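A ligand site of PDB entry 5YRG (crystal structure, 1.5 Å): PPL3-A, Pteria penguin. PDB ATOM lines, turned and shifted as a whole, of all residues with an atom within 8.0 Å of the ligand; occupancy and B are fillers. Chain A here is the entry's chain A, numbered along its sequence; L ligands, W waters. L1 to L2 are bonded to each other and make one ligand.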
ATOM      1  N   GLY A   9     -13.229  13.934   9.231  1.00  0.00           N
ATOM      2  CA  GLY A   9     -12.054  14.766   9.369  1.00  0.00           C
ATOM      3  C   GLY A   9     -11.093  14.623   8.215  1.00  0.00           C
ATOM      4  O   GLY A   9     -11.311  13.877   7.256  1.00  0.00           O
ATOM      5  N   PRO A  10      -9.969  15.342   8.295  1.00  0.00           N
ATOM      6  CA  PRO A  10      -8.994  15.346   7.207  1.00  0.00           C
ATOM      7  C   PRO A  10      -7.924  14.276   7.268  1.00  0.00           C
ATOM      8  O   PRO A  10      -7.098  14.228   6.357  1.00  0.00           O
ATOM      9  CB  PRO A  10      -8.354  16.736   7.370  1.00  0.00           C
ATOM     10  CG  PRO A  10      -8.435  16.988   8.820  1.00  0.00           C
ATOM     11  CD  PRO A  10      -9.730  16.428   9.265  1.00  0.00           C
ATOM     12  N   GLY A  11      -7.901  13.439   8.295  1.00  0.00           N
ATOM     13  CA  GLY A  11      -6.860  12.444   8.446  1.00  0.00           C
ATOM     14  C   GLY A  11      -7.077  11.268   7.518  1.00  0.00           C
ATOM     15  O   GLY A  11      -7.983  11.239   6.698  1.00  0.00           O
ATOM     16  N   GLY A  12      -6.193  10.283   7.678  1.00  0.00           N
ATOM     17  CA  GLY A  12      -6.276   9.082   6.884  1.00  0.00           C
ATOM     18  C   GLY A  12      -5.924   9.338   5.428  1.00  0.00           C
ATOM     19  O   GLY A  12      -5.380  10.377   5.057  1.00  0.00           O
ATOM     20  N   ASP A  13      -6.223   8.330   4.616  1.00  0.00           N
ATOM     21  CA  ASP A  13      -6.036   8.376   3.172  1.00  0.00           C
ATOM     22  C   ASP A  13      -7.390   8.274   2.485  1.00  0.00           C
ATOM     23  O   ASP A  13      -8.297   7.599   2.982  1.00  0.00           O
ATOM     24  CB  ASP A  13      -5.149   7.227   2.682  1.00  0.00           C
ATOM     25  CG  ASP A  13      -3.739   7.316   3.229  1.00  0.00           C
ATOM     26  OD1 ASP A  13      -3.023   8.290   2.908  1.00  0.00           O
ATOM     27  OD2 ASP A  13      -3.349   6.405   3.982  1.00  0.00           O
ATOM     28  N   THR A  38     -14.732   1.032  13.506  1.00  0.00           N
ATOM     29  CA  THR A  38     -13.325   1.100  13.137  1.00  0.00           C
ATOM     30  C   THR A  38     -13.001   0.708  11.697  1.00  0.00           C
ATOM     31  O   THR A  38     -11.925   1.054  11.212  1.00  0.00           O
ATOM     32  CB  THR A  38     -12.452   0.264  14.097  1.00  0.00           C
ATOM     33  OG1 THR A  38     -12.879  -1.093  14.111  1.00  0.00           O
ATOM     34  CG2 THR A  38     -12.527   0.810  15.504  1.00  0.00           C
ATOM     35  N   GLY A  53     -10.372   0.999   7.064  1.00  0.00           N
ATOM     36  CA  GLY A  53     -10.214   1.170   8.483  1.00  0.00           C
ATOM     37  C   GLY A  53      -9.364   0.067   9.074  1.00  0.00           C
ATOM     38  O   GLY A  53      -9.001  -0.901   8.403  1.00  0.00           O
ATOM     39  N   TRP A  54      -9.085   0.207  10.370  1.00  0.00           N
ATOM     40  CA  TRP A  54      -8.254  -0.712  11.140  1.00  0.00           C
ATOM     41  C   TRP A  54      -7.060  -1.186  10.307  1.00  0.00           C
ATOM     42  O   TRP A  54      -6.876  -2.377  10.024  1.00  0.00           O
ATOM     43  CB  TRP A  54      -9.049  -1.893  11.696  1.00  0.00           C
ATOM     44  CG  TRP A  54      -8.356  -2.504  12.850  1.00  0.00           C
ATOM     45  CD1 TRP A  54      -7.730  -3.716  12.869  1.00  0.00           C
ATOM     46  CD2 TRP A  54      -8.167  -1.926  14.142  1.00  0.00           C
ATOM     47  NE1 TRP A  54      -7.163  -3.936  14.107  1.00  0.00           N
ATOM     48  CE2 TRP A  54      -7.419  -2.845  14.910  1.00  0.00           C
ATOM     49  CE3 TRP A  54      -8.554  -0.717  14.731  1.00  0.00           C
ATOM     50  CZ2 TRP A  54      -7.072  -2.609  16.237  1.00  0.00           C
ATOM     51  CZ3 TRP A  54      -8.194  -0.475  16.058  1.00  0.00           C
ATOM     52  CH2 TRP A  54      -7.463  -1.420  16.785  1.00  0.00           C
ATOM     53  N   GLY A  55      -6.243  -0.206   9.937  1.00  0.00           N
ATOM     54  CA  GLY A  55      -5.144  -0.427   8.998  1.00  0.00           C
ATOM     55  C   GLY A  55      -4.256  -1.590   9.430  1.00  0.00           C
ATOM     56  O   GLY A  55      -3.804  -2.367   8.584  1.00  0.00           O
ATOM     57  N   ASN A  58      -1.416  -2.552  15.144  1.00  0.00           N
ATOM     58  CA  ASN A  58      -0.825  -1.520  15.989  1.00  0.00           C
ATOM     59  C   ASN A  58      -1.841  -0.454  16.339  1.00  0.00           C
ATOM     60  O   ASN A  58      -1.657   0.274  17.324  1.00  0.00           O
ATOM     61  CB  ASN A  58       0.382  -0.904  15.281  1.00  0.00           C
ATOM     62  CG  ASN A  58       1.481  -1.914  15.038  1.00  0.00           C
ATOM     63  OD1 ASN A  58       1.903  -2.612  15.952  1.00  0.00           O
ATOM     64  ND2 ASN A  58       1.908  -2.026  13.783  1.00  0.00           N
ATOM     65  N   CYS A  59      -2.941  -0.375  15.601  1.00  0.00           N
ATOM     66  CA  CYS A  59      -3.955   0.621  15.893  1.00  0.00           C
ATOM     67  C   CYS A  59      -4.544   0.483  17.294  1.00  0.00           C
ATOM     68  O   CYS A  59      -5.205   1.403  17.768  1.00  0.00           O
ATOM     69  CB  CYS A  59      -5.066   0.552  14.834  1.00  0.00           C
ATOM     70  SG  CYS A  59      -4.481   1.032  13.222  1.00  0.00           S
ATOM     71  N   GLN A  61      -2.971   0.825  19.765  1.00  0.00           N
ATOM     72  CA  GLN A  61      -2.358   1.890  20.561  1.00  0.00           C
ATOM     73  C   GLN A  61      -3.277   3.096  20.683  1.00  0.00           C
ATOM     74  O   GLN A  61      -3.118   3.879  21.632  1.00  0.00           O
ATOM     75  CB  GLN A  61      -1.042   2.322  19.925  1.00  0.00           C
ATOM     76  CG  GLN A  61       0.032   1.259  19.992  1.00  0.00           C
ATOM     77  CD  GLN A  61       1.059   1.391  18.881  1.00  0.00           C
ATOM     78  OE1 GLN A  61       0.965   2.257  18.004  1.00  0.00           O
ATOM     79  NE2 GLN A  61       2.039   0.509  18.900  1.00  0.00           N
ATOM     80  N   TRP A  62      -4.234   3.264  19.768  1.00  0.00           N
ATOM     81  CA  TRP A  62      -5.015   4.495  19.700  1.00  0.00           C
ATOM     82  C   TRP A  62      -6.513   4.309  19.904  1.00  0.00           C
ATOM     83  O   TRP A  62      -7.191   5.301  20.192  1.00  0.00           O
ATOM     84  CB  TRP A  62      -4.793   5.185  18.352  1.00  0.00           C
ATOM     85  CG  TRP A  62      -3.349   5.232  17.992  1.00  0.00           C
ATOM     86  CD1 TRP A  62      -2.732   4.561  16.982  1.00  0.00           C
ATOM     87  CD2 TRP A  62      -2.329   5.976  18.666  1.00  0.00           C
ATOM     88  NE1 TRP A  62      -1.384   4.852  16.975  1.00  0.00           N
ATOM     89  CE2 TRP A  62      -1.111   5.716  17.998  1.00  0.00           C
ATOM     90  CE3 TRP A  62      -2.328   6.839  19.763  1.00  0.00           C
ATOM     91  CZ2 TRP A  62       0.085   6.288  18.396  1.00  0.00           C
ATOM     92  CZ3 TRP A  62      -1.133   7.411  20.161  1.00  0.00           C
ATOM     93  CH2 TRP A  62       0.063   7.133  19.480  1.00  0.00           C
ATOM     94  N   SER A  63      -7.034   3.100  19.759  1.00  0.00           N
ATOM     95  CA  SER A  63      -8.454   2.850  20.033  1.00  0.00           C
ATOM     96  C   SER A  63      -8.648   1.353  20.160  1.00  0.00           C
ATOM     97  O   SER A  63      -7.791   0.549  19.791  1.00  0.00           O
ATOM     98  CB  SER A  63      -9.369   3.431  18.945  1.00  0.00           C
ATOM     99  OG  SER A  63      -9.454   2.583  17.800  1.00  0.00           O
ATOM    100  N   LYS A  88     -13.807  14.584  14.332  1.00  0.00           N
ATOM    101  CA  LYS A  88     -12.506  14.309  13.730  1.00  0.00           C
ATOM    102  C   LYS A  88     -12.572  13.006  12.931  1.00  0.00           C
ATOM    103  O   LYS A  88     -11.942  12.892  11.863  1.00  0.00           O
ATOM    104  CB  LYS A  88     -11.453  14.243  14.823  1.00  0.00           C
ATOM    105  CG  LYS A  88     -10.017  14.158  14.363  1.00  0.00           C
ATOM    106  CD  LYS A  88      -9.077  14.222  15.568  1.00  0.00           C
ATOM    107  CE  LYS A  88      -7.620  14.025  15.173  1.00  0.00           C
ATOM    108  NZ  LYS A  88      -6.727  14.075  16.362  1.00  0.00           N
ATOM    109  N   TYR A  89     -13.336  12.036  13.427  1.00  0.00           N
ATOM    110  CA  TYR A  89     -13.535  10.743  12.778  1.00  0.00           C
ATOM    111  C   TYR A  89     -15.021  10.476  12.703  1.00  0.00           C
ATOM    112  O   TYR A  89     -15.826  11.098  13.406  1.00  0.00           O
ATOM    113  CB  TYR A  89     -12.880   9.588  13.548  1.00  0.00           C
ATOM    114  CG  TYR A  89     -11.454   9.842  13.999  1.00  0.00           C
ATOM    115  CD1 TYR A  89     -10.442  10.043  13.085  1.00  0.00           C
ATOM    116  CD2 TYR A  89     -11.141   9.861  15.344  1.00  0.00           C
ATOM    117  CE1 TYR A  89      -9.124  10.265  13.520  1.00  0.00           C
ATOM    118  CE2 TYR A  89      -9.840  10.085  15.790  1.00  0.00           C
ATOM    119  CZ  TYR A  89      -8.848  10.282  14.862  1.00  0.00           C
ATOM    120  OH  TYR A  89      -7.550  10.479  15.290  1.00  0.00           O
ATOM    121  N   ARG A 128     -12.329   8.552   3.878  1.00  0.00           N
ATOM    122  CA  ARG A 128     -10.942   8.520   4.278  1.00  0.00           C
ATOM    123  C   ARG A 128     -10.800   7.511   5.390  1.00  0.00           C
ATOM    124  O   ARG A 128     -11.722   7.333   6.214  1.00  0.00           O
ATOM    125  CB  ARG A 128     -10.458   9.915   4.710  1.00  0.00           C
ATOM    126  CG  ARG A 128     -10.578  10.976   3.641  1.00  0.00           C
ATOM    127  CD  ARG A 128      -9.967  12.307   4.108  1.00  0.00           C
ATOM    128  NE  ARG A 128      -8.512  12.234   4.194  1.00  0.00           N
ATOM    129  CZ  ARG A 128      -7.684  12.468   3.176  1.00  0.00           C
ATOM    130  NH1 ARG A 128      -8.140  12.805   1.977  1.00  0.00           N
ATOM    131  NH2 ARG A 128      -6.370  12.380   3.365  1.00  0.00           N
ATOM    132  N   TRP A 129      -9.627   6.883   5.475  1.00  0.00           N
ATOM    133  CA  TRP A 129      -9.427   5.783   6.412  1.00  0.00           C
ATOM    134  C   TRP A 129      -7.980   5.704   6.846  1.00  0.00           C
ATOM    135  O   TRP A 129      -7.059   6.116   6.139  1.00  0.00           O
ATOM    136  CB  TRP A 129      -9.830   4.444   5.785  1.00  0.00           C
ATOM    137  CG  TRP A 129      -8.913   4.041   4.700  1.00  0.00           C
ATOM    138  CD1 TRP A 129      -8.870   4.522   3.438  1.00  0.00           C
ATOM    139  CD2 TRP A 129      -7.870   3.054   4.793  1.00  0.00           C
ATOM    140  NE1 TRP A 129      -7.876   3.905   2.718  1.00  0.00           N
ATOM    141  CE2 TRP A 129      -7.251   2.997   3.534  1.00  0.00           C
ATOM    142  CE3 TRP A 129      -7.406   2.218   5.815  1.00  0.00           C
ATOM    143  CZ2 TRP A 129      -6.186   2.122   3.259  1.00  0.00           C
ATOM    144  CZ3 TRP A 129      -6.334   1.349   5.529  1.00  0.00           C
ATOM    145  CH2 TRP A 129      -5.739   1.318   4.262  1.00  0.00           C
ATOM    146  N   GLY A 130      -7.790   5.095   8.018  1.00  0.00           N
ATOM    147  CA  GLY A 130      -6.490   4.723   8.534  1.00  0.00           C
ATOM    148  C   GLY A 130      -6.700   3.672   9.596  1.00  0.00           C
ATOM    149  O   GLY A 130      -7.173   2.573   9.306  1.00  0.00           O
ATOM    150  N   CYS A 131      -6.343   4.002  10.837  1.00  0.00           N
ATOM    151  CA  CYS A 131      -6.687   3.115  11.947  1.00  0.00           C
ATOM    152  C   CYS A 131      -8.186   3.016  12.127  1.00  0.00           C
ATOM    153  O   CYS A 131      -8.686   2.038  12.677  1.00  0.00           O
ATOM    154  CB  CYS A 131      -6.033   3.611  13.234  1.00  0.00           C
ATOM    155  SG  CYS A 131      -4.287   3.031  13.407  1.00  0.00           S
ATOM    156  N   ARG A 132      -8.926   4.034  11.685  1.00  0.00           N
ATOM    157  CA  ARG A 132     -10.377   3.959  11.743  1.00  0.00           C
ATOM    158  C   ARG A 132     -10.945   4.659  10.520  1.00  0.00           C
ATOM    159  O   ARG A 132     -10.302   4.787   9.472  1.00  0.00           O
ATOM    160  CB  ARG A 132     -10.852   4.514  13.084  1.00  0.00           C
ATOM    161  CG  ARG A 132     -10.399   5.910  13.363  1.00  0.00           C
ATOM    162  CD  ARG A 132     -10.673   6.229  14.807  1.00  0.00           C
ATOM    163  NE  ARG A 132     -12.110   6.464  15.008  1.00  0.00           N
ATOM    164  CZ  ARG A 132     -12.643   6.882  16.145  1.00  0.00           C
ATOM    165  NH1 ARG A 132     -11.885   7.123  17.196  1.00  0.00           N
ATOM    166  NH2 ARG A 132     -13.940   7.105  16.190  1.00  0.00           N
ATOM    167  N   ILE A 133     -12.218   5.049  10.603  1.00  0.00           N
ATOM    168  CA  ILE A 133     -12.918   5.667   9.495  1.00  0.00           C
ATOM    169  C   ILE A 133     -12.860   7.171   9.732  1.00  0.00           C
ATOM    170  O   ILE A 133     -13.596   7.701  10.574  1.00  0.00           O
ATOM    171  CB  ILE A 133     -14.363   5.179   9.387  1.00  0.00           C
ATOM    172  CG1 ILE A 133     -14.383   3.659   9.298  1.00  0.00           C
ATOM    173  CG2 ILE A 133     -14.997   5.776   8.157  1.00  0.00           C
ATOM    174  CD1 ILE A 133     -15.757   3.133   9.400  1.00  0.00           C
ATOM    175  N   ASP A 134     -11.997   7.866   8.976  1.00  0.00           N
ATOM    176  CA  ASP A 134     -11.844   9.291   9.176  1.00  0.00           C
ATOM    177  C   ASP A 134     -13.055  10.064   8.671  1.00  0.00           C
ATOM    178  O   ASP A 134     -13.440  11.065   9.276  1.00  0.00           O
ATOM    179  CB  ASP A 134     -10.562   9.780   8.509  1.00  0.00           C
ATOM    180  CG  ASP A 134      -9.315   9.297   9.239  1.00  0.00           C
ATOM    181  OD1 ASP A 134      -8.886   8.159   8.962  1.00  0.00           O
ATOM    182  OD2 ASP A 134      -8.818  10.020  10.143  1.00  0.00           O
ATOM    183  N   GLY A 135     -13.710   9.592   7.616  1.00  0.00           N
ATOM    184  CA  GLY A 135     -14.926  10.229   7.156  1.00  0.00           C
ATOM    185  C   GLY A 135     -15.547   9.402   6.049  1.00  0.00           C
ATOM    186  O   GLY A 135     -14.912   8.488   5.508  1.00  0.00           O
HETATM  187  C1  LIG L   1      -2.406  10.164  16.524  1.00  0.00           C
HETATM  188  C2  LIG L   1      -3.836   9.662  16.644  1.00  0.00           C
HETATM  189  C3  LIG L   1      -4.158   8.788  15.459  1.00  0.00           C
HETATM  190  C4  LIG L   1      -3.111   7.689  15.390  1.00  0.00           C
HETATM  191  C5  LIG L   1      -3.356   6.745  14.235  1.00  0.00           C
HETATM  192  C6  LIG L   1      -1.434   9.024  16.296  1.00  0.00           C
HETATM  193  O1  LIG L   1      -0.185   9.553  15.980  1.00  0.00           O
HETATM  194  O2  LIG L   1      -2.025  10.828  17.700  1.00  0.00           O
HETATM  195  O3  LIG L   1      -4.754  10.726  16.684  1.00  0.00           O
HETATM  196  O4  LIG L   1      -5.444   8.197  15.609  1.00  0.00           O
HETATM  197  O5  LIG L   1      -1.820   8.216  15.205  1.00  0.00           O
HETATM  198  O6  LIG L   1      -3.346   7.593  13.124  1.00  0.00           O
HETATM  199  C1  LG2 L   2      -3.741   6.961  11.894  1.00  0.00           C
HETATM  200  C2  LG2 L   2      -3.439   7.779  10.630  1.00  0.00           C
HETATM  201  C3  LG2 L   2      -4.226   9.037  10.683  1.00  0.00           C
HETATM  202  C4  LG2 L   2      -5.693   8.713  10.796  1.00  0.00           C
HETATM  203  C5  LG2 L   2      -5.944   7.717  11.913  1.00  0.00           C
HETATM  204  C6  LG2 L   2      -7.405   7.307  11.978  1.00  0.00           C
HETATM  205  O1  LG2 L   2      -2.069   8.090  10.555  1.00  0.00           O
HETATM  206  O2  LG2 L   2      -3.976   9.845   9.611  1.00  0.00           O
HETATM  207  O3  LG2 L   2      -6.366   9.911  11.080  1.00  0.00           O
HETATM  208  O4  LG2 L   2      -5.116   6.583  11.817  1.00  0.00           O
HETATM  209  O5  LG2 L   2      -7.680   6.850  10.709  1.00  0.00           O
HETATM  210  O   HOH W   1       0.239  10.955  19.672  1.00  0.00           O
HETATM  211  O   HOH W   2      -3.303  12.855  10.776  1.00  0.00           O
HETATM  212  O   HOH W   3      -7.322   6.032  15.744  1.00  0.00           O
HETATM  213  O   HOH W   4      -3.527  10.742  19.864  1.00  0.00           O
HETATM  214  O   HOH W   5      -5.659  11.975  12.640  1.00  0.00           O
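N of Cys 131 lies within hydrogen-bond range of O4 of LG2 L2, 3.0 Å away.
An oxygen (O2) of LG2 L2 sits at hydrogen-bond distance from the backbone NH (N) of Gly 12 (3.0 Å).
OH of Tyr 89 lies within hydrogen-bond range of O4 of LIG L1 (3.1 Å).
The backbone NH of Arg 132 sits at hydrogen-bond distance from an oxygen (O5) of LG2 L2.
O5 of LG2 L2 sits at hydrogen-bond distance from OD1 of Asp 134, 2.5 Å away.
An oxygen (O5) of LG2 L2 lies within hydrogen-bond range of the backbone NH (N) of Gly 130, at 3.2 Å.
The backbone NH (N) of Gly 9 sits at hydrogen-bond distance from the backbone carbonyl oxygen (O) of Asp 134 (2.9 Å).
The guanidinium group (NE) of Arg 128 lies within hydrogen-bond range of the backbone carbonyl oxygen (O) of Gly 11.
O of Cys 131 lies within hydrogen-bond range of N of Trp 54 (3.0 Å).
The backbone carbonyl oxygen of Lys 88 is in hydrogen-bond range of the backbone NH of Gly 9 (3.1 Å).
The guanidinium group (NH2) of Arg 128 is in hydrogen-bond range of the backbone carbonyl oxygen (O) of Gly 12, 2.8 Å away.
O of Gly 130 is in hydrogen-bond range of N of Trp 54 (3.2 Å).
The backbone NH (N) of Gly 55 is in hydrogen-bond range of the backbone carbonyl oxygen (O) of Gly 130 (3.0 Å).
The backbone NH (N) of Gly 130 is in hydrogen-bond range of the side-chain carboxylate (OD1) of Asp 134, 3.4 Å away.
Gly 11 touches the ligand.
CD1 of Trp 62 touches C4 of LIG L1, 3.5 Å away.
NZ of Lys 88 touches O3 of LIG L1, 3.9 Å away.
Hydrophobic or aromatic side chains within 4 Å of the ligand: Trp 62 and Tyr 89.
Of the 24 residues printed, 9 come within 4 Å of the ligand.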
